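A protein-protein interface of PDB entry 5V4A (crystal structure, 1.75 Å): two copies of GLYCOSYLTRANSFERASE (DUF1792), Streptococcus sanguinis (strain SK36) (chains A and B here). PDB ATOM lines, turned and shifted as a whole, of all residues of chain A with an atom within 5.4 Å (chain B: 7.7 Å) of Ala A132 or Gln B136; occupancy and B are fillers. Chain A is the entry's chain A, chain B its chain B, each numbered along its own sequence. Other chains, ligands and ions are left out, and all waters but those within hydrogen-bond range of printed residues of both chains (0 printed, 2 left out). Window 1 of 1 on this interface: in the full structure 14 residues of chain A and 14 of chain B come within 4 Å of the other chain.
The backbone carbonyl oxygen (O) of Lys A135 sits close to the side-chain amide nitrogen (NE2) of Gln A139 (3.2 Å). The side-chain carboxylate (OD2) of Asp B16 is in salt-bridge range of the side-chain amino group (NZ) of Lys B133 (2.9 Å). O of Lys B135 lies close to OE1 of Gln B139.
The side-chain amide oxygen (OE1) of Gln A136 lies close to the side-chain amide oxygen (OE1) of Gln B136, 2.9 Å away.
Gly A129 touches Lys B133, and with the chains exchanged Lys A133 touches Gly B129. Ala A132 touches Gln B136, and with the chains exchanged Gln A136 touches Ala B132. Gln A136 touches its own counterpart, Gln B136. Gln A136 touches Gln B139, and with the chains exchanged Gln A139 touches Gln B136. Of the 16 pairs that touch across the chains among the printed residues, 11 have their exchanged pair printed and touching as well.
Of the 11 printed residues of chain A, 7 touch a printed residue of chain B. Printed residues of chain A that touch a printed residue of chain B: Val A128, Gly A129, Ala A132, Lys A133, Lys A135, Gln A136 and Gln A139. Hydrophobic or aromatic side chains of chain A that line the printed part of chain B: Val A128 and Ala A132. Hydrophobic or aromatic side chains of chain B that line the printed part of chain A: Leu B19 and Ala B132. Among the printed residues, no Asp or Glu carboxylate lies within 4 Å of a Lys or Arg side-chain nitrogen of the other chain.
Asp B16 touches Val A128. Val A128 touches Leu B19. Lys B133 touches Gly A129 (CD to CA, 3.8 Å). CG of Gln B136 touches O of Ala A132, at 3.5 Å. Gly B129 touches Lys A133. Lys B133 touches Lys A133. Gln B136 touches Lys A135 (NE2 to CB, 3.8 Å). Gln A136 touches Lys B135. Gln A139 touches Gln B136 (CG to OE1, 3.3 Å). OE1 of Gln A139 touches NE2 of Gln B139 (3.6 Å).
Ala A132 touches just these residues of chain B: Leu B19 and Gln B136. Printed residues of chain B within 4 Å of Gln A136: Ala B132 (3.7 Å), Lys B135 (3.5 Å), Gln B136 (2.9 Å) and Gln B139 (3.99 Å). Of the printed residues of chain A, Ala B132 touches Gln A136. Printed residues of chain A within 4 Å of Lys B133: Gly A129 (3.8 Å) and Lys A133 (3.8 Å). Of the printed residues of chain A, Lys B135 touches Gln A136. Gln B136 touches four residues of chain A. Lys B141 touches none of the printed residues of chain A. The nearest residue of chain A that does not touch Gln B136 is Lys A133 (5.1 Å). The nearest printed residue of chain A that does not touch Lys B135 is Gln A139 (7.0 Å).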
ATOM      1  N   SER A 127     -22.237  -9.275   0.124  1.00  0.00           N
ATOM      2  CA  SER A 127     -23.654  -9.008  -0.128  1.00  0.00           C
ATOM      3  C   SER A 127     -24.566  -9.815   0.786  1.00  0.00           C
ATOM      4  O   SER A 127     -25.591  -9.301   1.265  1.00  0.00           O
ATOM      5  CB  SER A 127     -23.988  -9.304  -1.587  1.00  0.00           C
ATOM      6  OG  SER A 127     -23.299  -8.431  -2.456  1.00  0.00           O
ATOM      7  N   VAL A 128     -24.197 -11.073   1.061  1.00  0.00           N
ATOM      8  CA  VAL A 128     -25.000 -11.928   1.930  1.00  0.00           C
ATOM      9  C   VAL A 128     -25.210 -11.268   3.283  1.00  0.00           C
ATOM     10  O   VAL A 128     -26.288 -11.368   3.880  1.00  0.00           O
ATOM     11  CB  VAL A 128     -24.343 -13.321   2.044  1.00  0.00           C
ATOM     12  CG1 VAL A 128     -22.989 -13.224   2.693  1.00  0.00           C
ATOM     13  CG2 VAL A 128     -25.222 -14.262   2.844  1.00  0.00           C
ATOM     14  N   GLY A 129     -24.171 -10.605   3.798  1.00  0.00           N
ATOM     15  CA  GLY A 129     -24.275  -9.961   5.092  1.00  0.00           C
ATOM     16  C   GLY A 129     -25.090  -8.695   5.004  1.00  0.00           C
ATOM     17  O   GLY A 129     -25.792  -8.343   5.956  1.00  0.00           O
ATOM     18  N   TYR A 130     -25.024  -7.999   3.863  1.00  0.00           N
ATOM     19  CA  TYR A 130     -25.829  -6.791   3.711  1.00  0.00           C
ATOM     20  C   TYR A 130     -27.315  -7.132   3.751  1.00  0.00           C
ATOM     21  O   TYR A 130     -28.100  -6.459   4.432  1.00  0.00           O
ATOM     22  CB  TYR A 130     -25.464  -6.045   2.417  1.00  0.00           C
ATOM     23  CG  TYR A 130     -24.018  -5.574   2.329  1.00  0.00           C
ATOM     24  CD1 TYR A 130     -23.259  -5.382   3.476  1.00  0.00           C
ATOM     25  CD2 TYR A 130     -23.419  -5.302   1.097  1.00  0.00           C
ATOM     26  CE1 TYR A 130     -21.950  -4.956   3.402  1.00  0.00           C
ATOM     27  CE2 TYR A 130     -22.103  -4.856   1.017  1.00  0.00           C
ATOM     28  CZ  TYR A 130     -21.367  -4.699   2.188  1.00  0.00           C
ATOM     29  OH  TYR A 130     -20.058  -4.264   2.151  1.00  0.00           O
ATOM     30  N   PHE A 131     -27.728  -8.171   3.009  1.00  0.00           N
ATOM     31  CA  PHE A 131     -29.130  -8.578   3.051  1.00  0.00           C
ATOM     32  C   PHE A 131     -29.522  -9.116   4.428  1.00  0.00           C
ATOM     33  O   PHE A 131     -30.679  -8.967   4.839  1.00  0.00           O
ATOM     34  CB  PHE A 131     -29.437  -9.624   1.966  1.00  0.00           C
ATOM     35  CG  PHE A 131     -29.447  -9.067   0.562  1.00  0.00           C
ATOM     36  CD1 PHE A 131     -30.414  -8.151   0.173  1.00  0.00           C
ATOM     37  CD2 PHE A 131     -28.500  -9.477  -0.375  1.00  0.00           C
ATOM     38  CE1 PHE A 131     -30.433  -7.639  -1.126  1.00  0.00           C
ATOM     39  CE2 PHE A 131     -28.511  -8.968  -1.673  1.00  0.00           C
ATOM     40  CZ  PHE A 131     -29.485  -8.038  -2.044  1.00  0.00           C
ATOM     41  N   ALA A 132     -28.592  -9.746   5.157  1.00  0.00           N
ATOM     42  CA  ALA A 132     -28.932 -10.201   6.502  1.00  0.00           C
ATOM     43  C   ALA A 132     -29.266  -9.026   7.416  1.00  0.00           C
ATOM     44  O   ALA A 132     -30.243  -9.075   8.171  1.00  0.00           O
ATOM     45  CB  ALA A 132     -27.792 -11.027   7.109  1.00  0.00           C
ATOM     46  N   LYS A 133     -28.466  -7.962   7.368  1.00  0.00           N
ATOM     47  CA  LYS A 133     -28.735  -6.816   8.243  1.00  0.00           C
ATOM     48  C   LYS A 133     -29.994  -6.072   7.817  1.00  0.00           C
ATOM     49  O   LYS A 133     -30.752  -5.573   8.664  1.00  0.00           O
ATOM     50  CB  LYS A 133     -27.528  -5.884   8.256  1.00  0.00           C
ATOM     51  CG  LYS A 133     -26.330  -6.467   9.010  1.00  0.00           C
ATOM     52  CD  LYS A 133     -25.360  -5.392   9.459  1.00  0.00           C
ATOM     53  CE  LYS A 133     -24.290  -5.142   8.451  1.00  0.00           C
ATOM     54  NZ  LYS A 133     -23.210  -4.280   8.972  1.00  0.00           N
ATOM     55  N   LEU A 134     -30.241  -6.001   6.508  1.00  0.00           N
ATOM     56  CA  LEU A 134     -31.490  -5.423   6.029  1.00  0.00           C
ATOM     57  C   LEU A 134     -32.680  -6.209   6.553  1.00  0.00           C
ATOM     58  O   LEU A 134     -33.635  -5.625   7.075  1.00  0.00           O
ATOM     59  CB  LEU A 134     -31.510  -5.396   4.500  1.00  0.00           C
ATOM     60  CG  LEU A 134     -30.781  -4.265   3.780  1.00  0.00           C
ATOM     61  CD1 LEU A 134     -30.372  -4.688   2.369  1.00  0.00           C
ATOM     62  CD2 LEU A 134     -31.662  -2.999   3.714  1.00  0.00           C
ATOM     63  N   LYS A 135     -32.624  -7.549   6.451  1.00  0.00           N
ATOM     64  CA  LYS A 135     -33.749  -8.357   6.912  1.00  0.00           C
ATOM     65  C   LYS A 135     -34.008  -8.154   8.394  1.00  0.00           C
ATOM     66  O   LYS A 135     -35.164  -8.187   8.820  1.00  0.00           O
ATOM     67  CB  LYS A 135     -33.538  -9.852   6.630  1.00  0.00           C
ATOM     68  CG  LYS A 135     -33.568 -10.236   5.142  1.00  0.00           C
ATOM     69  CD  LYS A 135     -33.504 -11.721   4.995  1.00  0.00           C
ATOM     70  CE  LYS A 135     -33.607 -12.133   3.551  1.00  0.00           C
ATOM     71  NZ  LYS A 135     -33.126 -13.535   3.456  1.00  0.00           N
ATOM     72  N   GLN A 136     -32.960  -7.902   9.179  1.00  0.00           N
ATOM     73  CA  GLN A 136     -33.124  -7.699  10.612  1.00  0.00           C
ATOM     74  C   GLN A 136     -33.899  -6.418  10.920  1.00  0.00           C
ATOM     75  O   GLN A 136     -34.472  -6.296  12.006  1.00  0.00           O
ATOM     76  CB  GLN A 136     -31.749  -7.664  11.287  1.00  0.00           C
ATOM     77  CG  GLN A 136     -31.775  -7.804  12.814  1.00  0.00           C
ATOM     78  CD  GLN A 136     -32.247  -9.167  13.284  1.00  0.00           C
ATOM     79  OE1 GLN A 136     -32.138 -10.158  12.567  1.00  0.00           O
ATOM     80  NE2 GLN A 136     -32.790  -9.217  14.490  1.00  0.00           N
ATOM     81  N   GLN A 139     -37.434  -7.968  10.669  1.00  0.00           N
ATOM     82  CA  GLN A 139     -37.711  -9.274  11.255  1.00  0.00           C
ATOM     83  C   GLN A 139     -38.706  -9.144  12.403  1.00  0.00           C
ATOM     84  O   GLN A 139     -38.509  -8.340  13.316  1.00  0.00           O
ATOM     85  CB  GLN A 139     -36.420  -9.923  11.769  1.00  0.00           C
ATOM     86  CG  GLN A 139     -35.533 -10.525  10.714  1.00  0.00           C
ATOM     87  CD  GLN A 139     -36.283 -11.477   9.821  1.00  0.00           C
ATOM     88  OE1 GLN A 139     -36.570 -12.617  10.205  1.00  0.00           O
ATOM     89  NE2 GLN A 139     -36.628 -11.011   8.623  1.00  0.00           N
ATOM     90  N   LEU B  15     -18.979 -14.454   9.891  1.00  0.00           N
ATOM     91  CA  LEU B  15     -20.430 -14.541   9.922  1.00  0.00           C
ATOM     92  C   LEU B  15     -20.997 -14.653   8.514  1.00  0.00           C
ATOM     93  O   LEU B  15     -21.971 -15.380   8.288  1.00  0.00           O
ATOM     94  CB  LEU B  15     -21.006 -13.320  10.632  1.00  0.00           C
ATOM     95  CG  LEU B  15     -20.731 -13.213  12.134  1.00  0.00           C
ATOM     96  CD1 LEU B  15     -21.344 -11.922  12.626  1.00  0.00           C
ATOM     97  CD2 LEU B  15     -21.346 -14.373  12.878  1.00  0.00           C
ATOM     98  N   ASP B  16     -20.438 -13.885   7.571  1.00  0.00           N
ATOM     99  CA  ASP B  16     -20.927 -13.958   6.197  1.00  0.00           C
ATOM    100  C   ASP B  16     -20.716 -15.346   5.617  1.00  0.00           C
ATOM    101  O   ASP B  16     -21.547 -15.830   4.843  1.00  0.00           O
ATOM    102  CB  ASP B  16     -20.230 -12.943   5.296  1.00  0.00           C
ATOM    103  CG  ASP B  16     -20.662 -11.514   5.553  1.00  0.00           C
ATOM    104  OD1 ASP B  16     -20.154 -10.626   4.838  1.00  0.00           O
ATOM    105  OD2 ASP B  16     -21.513 -11.277   6.431  1.00  0.00           O
ATOM    106  N   LEU B  19     -23.449 -17.451   6.992  1.00  0.00           N
ATOM    107  CA  LEU B  19     -24.703 -17.121   6.328  1.00  0.00           C
ATOM    108  C   LEU B  19     -24.717 -17.647   4.895  1.00  0.00           C
ATOM    109  O   LEU B  19     -25.740 -18.159   4.425  1.00  0.00           O
ATOM    110  CB  LEU B  19     -24.932 -15.611   6.354  1.00  0.00           C
ATOM    111  CG  LEU B  19     -25.264 -15.021   7.730  1.00  0.00           C
ATOM    112  CD1 LEU B  19     -25.076 -13.514   7.734  1.00  0.00           C
ATOM    113  CD2 LEU B  19     -26.682 -15.393   8.145  1.00  0.00           C
ATOM    114  N   GLY B 129     -24.174  -4.545  14.328  1.00  0.00           N
ATOM    115  CA  GLY B 129     -24.293  -5.303  13.090  1.00  0.00           C
ATOM    116  C   GLY B 129     -23.870  -6.744  13.257  1.00  0.00           C
ATOM    117  O   GLY B 129     -24.437  -7.637  12.609  1.00  0.00           O
ATOM    118  N   TYR B 130     -22.884  -6.990  14.125  1.00  0.00           N
ATOM    119  CA  TYR B 130     -22.472  -8.361  14.421  1.00  0.00           C
ATOM    120  C   TYR B 130     -23.618  -9.131  15.060  1.00  0.00           C
ATOM    121  O   TYR B 130     -23.969 -10.223  14.607  1.00  0.00           O
ATOM    122  CB  TYR B 130     -21.247  -8.366  15.347  1.00  0.00           C
ATOM    123  CG  TYR B 130     -20.037  -7.666  14.776  1.00  0.00           C
ATOM    124  CD1 TYR B 130     -19.857  -7.554  13.402  1.00  0.00           C
ATOM    125  CD2 TYR B 130     -19.096  -7.075  15.609  1.00  0.00           C
ATOM    126  CE1 TYR B 130     -18.749  -6.895  12.872  1.00  0.00           C
ATOM    127  CE2 TYR B 130     -17.993  -6.415  15.094  1.00  0.00           C
ATOM    128  CZ  TYR B 130     -17.835  -6.318  13.720  1.00  0.00           C
ATOM    129  OH  TYR B 130     -16.739  -5.653  13.228  1.00  0.00           O
ATOM    130  N   PHE B 131     -24.254  -8.552  16.087  1.00  0.00           N
ATOM    131  CA  PHE B 131     -25.368  -9.247  16.727  1.00  0.00           C
ATOM    132  C   PHE B 131     -26.540  -9.425  15.778  1.00  0.00           C
ATOM    133  O   PHE B 131     -27.266 -10.418  15.879  1.00  0.00           O
ATOM    134  CB  PHE B 131     -25.838  -8.506  17.980  1.00  0.00           C
ATOM    135  CG  PHE B 131     -24.891  -8.610  19.142  1.00  0.00           C
ATOM    136  CD1 PHE B 131     -24.702  -9.817  19.797  1.00  0.00           C
ATOM    137  CD2 PHE B 131     -24.178  -7.500  19.564  1.00  0.00           C
ATOM    138  CE1 PHE B 131     -23.831  -9.908  20.871  1.00  0.00           C
ATOM    139  CE2 PHE B 131     -23.301  -7.584  20.618  1.00  0.00           C
ATOM    140  CZ  PHE B 131     -23.130  -8.786  21.282  1.00  0.00           C
ATOM    141  N   ALA B 132     -26.752  -8.477  14.858  1.00  0.00           N
ATOM    142  CA  ALA B 132     -27.827  -8.634  13.892  1.00  0.00           C
ATOM    143  C   ALA B 132     -27.577  -9.838  12.981  1.00  0.00           C
ATOM    144  O   ALA B 132     -28.485 -10.637  12.728  1.00  0.00           O
ATOM    145  CB  ALA B 132     -27.974  -7.348  13.077  1.00  0.00           C
ATOM    146  N   LYS B 133     -26.349  -9.988  12.482  1.00  0.00           N
ATOM    147  CA  LYS B 133     -26.047 -11.123  11.609  1.00  0.00           C
ATOM    148  C   LYS B 133     -26.036 -12.443  12.381  1.00  0.00           C
ATOM    149  O   LYS B 133     -26.422 -13.476  11.831  1.00  0.00           O
ATOM    150  CB  LYS B 133     -24.717 -10.894  10.902  1.00  0.00           C
ATOM    151  CG  LYS B 133     -24.799  -9.818   9.862  1.00  0.00           C
ATOM    152  CD  LYS B 133     -23.673  -9.938   8.886  1.00  0.00           C
ATOM    153  CE  LYS B 133     -22.510  -9.120   9.326  1.00  0.00           C
ATOM    154  NZ  LYS B 133     -21.477  -8.982   8.280  1.00  0.00           N
ATOM    155  N   LEU B 134     -25.624 -12.423  13.656  1.00  0.00           N
ATOM    156  CA  LEU B 134     -25.729 -13.624  14.482  1.00  0.00           C
ATOM    157  C   LEU B 134     -27.186 -14.058  14.628  1.00  0.00           C
ATOM    158  O   LEU B 134     -27.515 -15.237  14.455  1.00  0.00           O
ATOM    159  CB  LEU B 134     -25.087 -13.383  15.852  1.00  0.00           C
ATOM    160  CG  LEU B 134     -23.565 -13.444  15.916  1.00  0.00           C
ATOM    161  CD1 LEU B 134     -23.088 -12.609  17.106  1.00  0.00           C
ATOM    162  CD2 LEU B 134     -23.088 -14.905  16.042  1.00  0.00           C
ATOM    163  N   LYS B 135     -28.081 -13.105  14.922  1.00  0.00           N
ATOM    164  CA  LYS B 135     -29.493 -13.431  15.092  1.00  0.00           C
ATOM    165  C   LYS B 135     -30.080 -14.021  13.816  1.00  0.00           C
ATOM    166  O   LYS B 135     -30.998 -14.849  13.871  1.00  0.00           O
ATOM    167  CB  LYS B 135     -30.273 -12.177  15.511  1.00  0.00           C
ATOM    168  CG  LYS B 135     -29.951 -11.610  16.910  1.00  0.00           C
ATOM    169  CD  LYS B 135     -30.830 -10.362  17.190  1.00  0.00           C
ATOM    170  CE  LYS B 135     -30.673  -9.843  18.609  1.00  0.00           C
ATOM    171  NZ  LYS B 135     -31.284  -8.482  18.793  1.00  0.00           N
ATOM    172  N   GLN B 136     -29.565 -13.604  12.660  1.00  0.00           N
ATOM    173  CA  GLN B 136     -30.062 -14.128  11.390  1.00  0.00           C
ATOM    174  C   GLN B 136     -29.738 -15.604  11.212  1.00  0.00           C
ATOM    175  O   GLN B 136     -30.396 -16.282  10.411  1.00  0.00           O
ATOM    176  CB  GLN B 136     -29.487 -13.302  10.246  1.00  0.00           C
ATOM    177  CG  GLN B 136     -30.241 -11.985  10.036  1.00  0.00           C
ATOM    178  CD  GLN B 136     -31.669 -12.206   9.570  1.00  0.00           C
ATOM    179  OE1 GLN B 136     -32.615 -11.906  10.290  1.00  0.00           O
ATOM    180  NE2 GLN B 136     -31.831 -12.740   8.355  1.00  0.00           N
ATOM    181  N   LEU B 137     -28.734 -16.113  11.930  1.00  0.00           N
ATOM    182  CA  LEU B 137     -28.425 -17.542  11.867  1.00  0.00           C
ATOM    183  C   LEU B 137     -29.552 -18.389  12.454  1.00  0.00           C
ATOM    184  O   LEU B 137     -29.799 -19.504  11.972  1.00  0.00           O
ATOM    185  CB  LEU B 137     -27.109 -17.827  12.588  1.00  0.00           C
ATOM    186  CG  LEU B 137     -25.849 -17.293  11.906  1.00  0.00           C
ATOM    187  CD1 LEU B 137     -24.628 -17.606  12.757  1.00  0.00           C
ATOM    188  CD2 LEU B 137     -25.704 -17.903  10.533  1.00  0.00           C
ATOM    189  N   TRP B 138     -30.271 -17.877  13.461  1.00  0.00           N
ATOM    190  CA  TRP B 138     -31.353 -18.636  14.073  1.00  0.00           C
ATOM    191  C   TRP B 138     -32.745 -18.047  13.849  1.00  0.00           C
ATOM    192  O   TRP B 138     -33.721 -18.600  14.371  1.00  0.00           O
ATOM    193  CB  TRP B 138     -31.085 -18.830  15.577  1.00  0.00           C
ATOM    194  CG  TRP B 138     -30.755 -17.587  16.375  1.00  0.00           C
ATOM    195  CD1 TRP B 138     -31.617 -16.628  16.814  1.00  0.00           C
ATOM    196  CD2 TRP B 138     -29.459 -17.210  16.848  1.00  0.00           C
ATOM    197  NE1 TRP B 138     -30.936 -15.670  17.539  1.00  0.00           N
ATOM    198  CE2 TRP B 138     -29.607 -16.000  17.564  1.00  0.00           C
ATOM    199  CE3 TRP B 138     -28.179 -17.774  16.726  1.00  0.00           C
ATOM    200  CZ2 TRP B 138     -28.530 -15.346  18.155  1.00  0.00           C
ATOM    201  CZ3 TRP B 138     -27.110 -17.120  17.316  1.00  0.00           C
ATOM    202  CH2 TRP B 138     -27.292 -15.921  18.019  1.00  0.00           C
ATOM    203  N   GLN B 139     -32.877 -16.978  13.058  1.00  0.00           N
ATOM    204  CA  GLN B 139     -34.187 -16.379  12.814  1.00  0.00           C
ATOM    205  C   GLN B 139     -35.142 -17.397  12.197  1.00  0.00           C
ATOM    206  O   GLN B 139     -34.844 -17.986  11.153  1.00  0.00           O
ATOM    207  CB  GLN B 139     -34.059 -15.163  11.894  1.00  0.00           C
ATOM    208  CG  GLN B 139     -33.535 -13.895  12.553  1.00  0.00           C
ATOM    209  CD  GLN B 139     -34.301 -13.504  13.795  1.00  0.00           C
ATOM    210  OE1 GLN B 139     -33.770 -13.552  14.908  1.00  0.00           O
ATOM    211  NE2 GLN B 139     -35.558 -13.106  13.615  1.00  0.00           N
ATOM    212  N   ASP B 140     -36.292 -17.590  12.846  1.00  0.00           N
ATOM    213  CA  ASP B 140     -37.354 -18.485  12.376  1.00  0.00           C
ATOM    214  C   ASP B 140     -36.899 -19.942  12.316  1.00  0.00           C
ATOM    215  O   ASP B 140     -37.392 -20.718  11.495  1.00  0.00           O
ATOM    216  CB  ASP B 140     -37.903 -18.050  11.012  1.00  0.00           C
ATOM    217  CG  ASP B 140     -38.591 -16.704  11.070  1.00  0.00           C
ATOM    218  OD1 ASP B 140     -39.571 -16.575  11.838  1.00  0.00           O
ATOM    219  OD2 ASP B 140     -38.158 -15.784  10.338  1.00  0.00           O
ATOM    220  N   LYS B 141     -35.945 -20.319  13.162  1.00  0.00           N
ATOM    221  CA  LYS B 141     -35.459 -21.688  13.241  1.00  0.00           C
ATOM    222  C   LYS B 141     -35.953 -22.350  14.521  1.00  0.00           C
ATOM    223  O   LYS B 141     -36.089 -21.703  15.558  1.00  0.00           O
ATOM    224  CB  LYS B 141     -33.931 -21.731  13.210  1.00  0.00           C
ATOM    225  CG  LYS B 141     -33.291 -21.150  11.971  1.00  0.00           C
ATOM    226  CD  LYS B 141     -33.567 -21.993  10.741  1.00  0.00           C
ATOM    227  CE  LYS B 141     -32.701 -21.518   9.603  1.00  0.00           C
ATOM    228  NZ  LYS B 141     -31.279 -21.354  10.020  1.00  0.00           N
ATOM    229  N   LEU B 159     -32.262 -12.111  22.991  1.00  0.00           N
ATOM    230  CA  LEU B 159     -31.298 -12.679  22.039  1.00  0.00           C
ATOM    231  C   LEU B 159     -31.930 -13.694  21.087  1.00  0.00           C
ATOM    232  O   LEU B 159     -31.650 -13.689  19.879  1.00  0.00           O
ATOM    233  CB  LEU B 159     -30.146 -13.331  22.808  1.00  0.00           C
ATOM    234  CG  LEU B 159     -28.961 -13.869  22.004  1.00  0.00           C
ATOM    235  CD1 LEU B 159     -28.290 -12.774  21.196  1.00  0.00           C
ATOM    236  CD2 LEU B 159     -27.973 -14.543  22.934  1.00  0.00           C
ATOM    237  N   LEU B 195     -31.743 -26.679  14.594  1.00  0.00           N
ATOM    238  CA  LEU B 195     -30.391 -26.147  14.594  1.00  0.00           C
ATOM    239  C   LEU B 195     -29.851 -26.215  16.017  1.00  0.00           C
ATOM    240  O   LEU B 195     -30.507 -25.757  16.957  1.00  0.00           O
ATOM    241  CB  LEU B 195     -30.397 -24.706  14.070  1.00  0.00           C
ATOM    242  CG  LEU B 195     -29.137 -23.840  14.183  1.00  0.00           C
ATOM    243  CD1 LEU B 195     -27.966 -24.468  13.454  1.00  0.00           C
ATOM    244  CD2 LEU B 195     -29.386 -22.430  13.653  1.00  0.00           C
ATOM    245  N   ARG B 217     -26.278 -29.953  12.010  1.00  0.00           N
ATOM    246  CA  ARG B 217     -25.686 -28.628  11.915  1.00  0.00           C
ATOM    247  C   ARG B 217     -25.642 -28.052  13.327  1.00  0.00           C
ATOM    248  O   ARG B 217     -26.651 -28.068  14.034  1.00  0.00           O
ATOM    249  CB  ARG B 217     -26.501 -27.711  11.000  1.00  0.00           C
ATOM    250  CG  ARG B 217     -25.877 -26.369  10.743  1.00  0.00           C
ATOM    251  CD  ARG B 217     -26.796 -25.546   9.866  1.00  0.00           C
ATOM    252  NE  ARG B 217     -26.288 -24.193   9.692  1.00  0.00           N
ATOM    253  CZ  ARG B 217     -27.039 -23.093   9.700  1.00  0.00           C
ATOM    254  NH1 ARG B 217     -28.355 -23.159   9.889  1.00  0.00           N
ATOM    255  NH2 ARG B 217     -26.457 -21.925   9.526  1.00  0.00           N
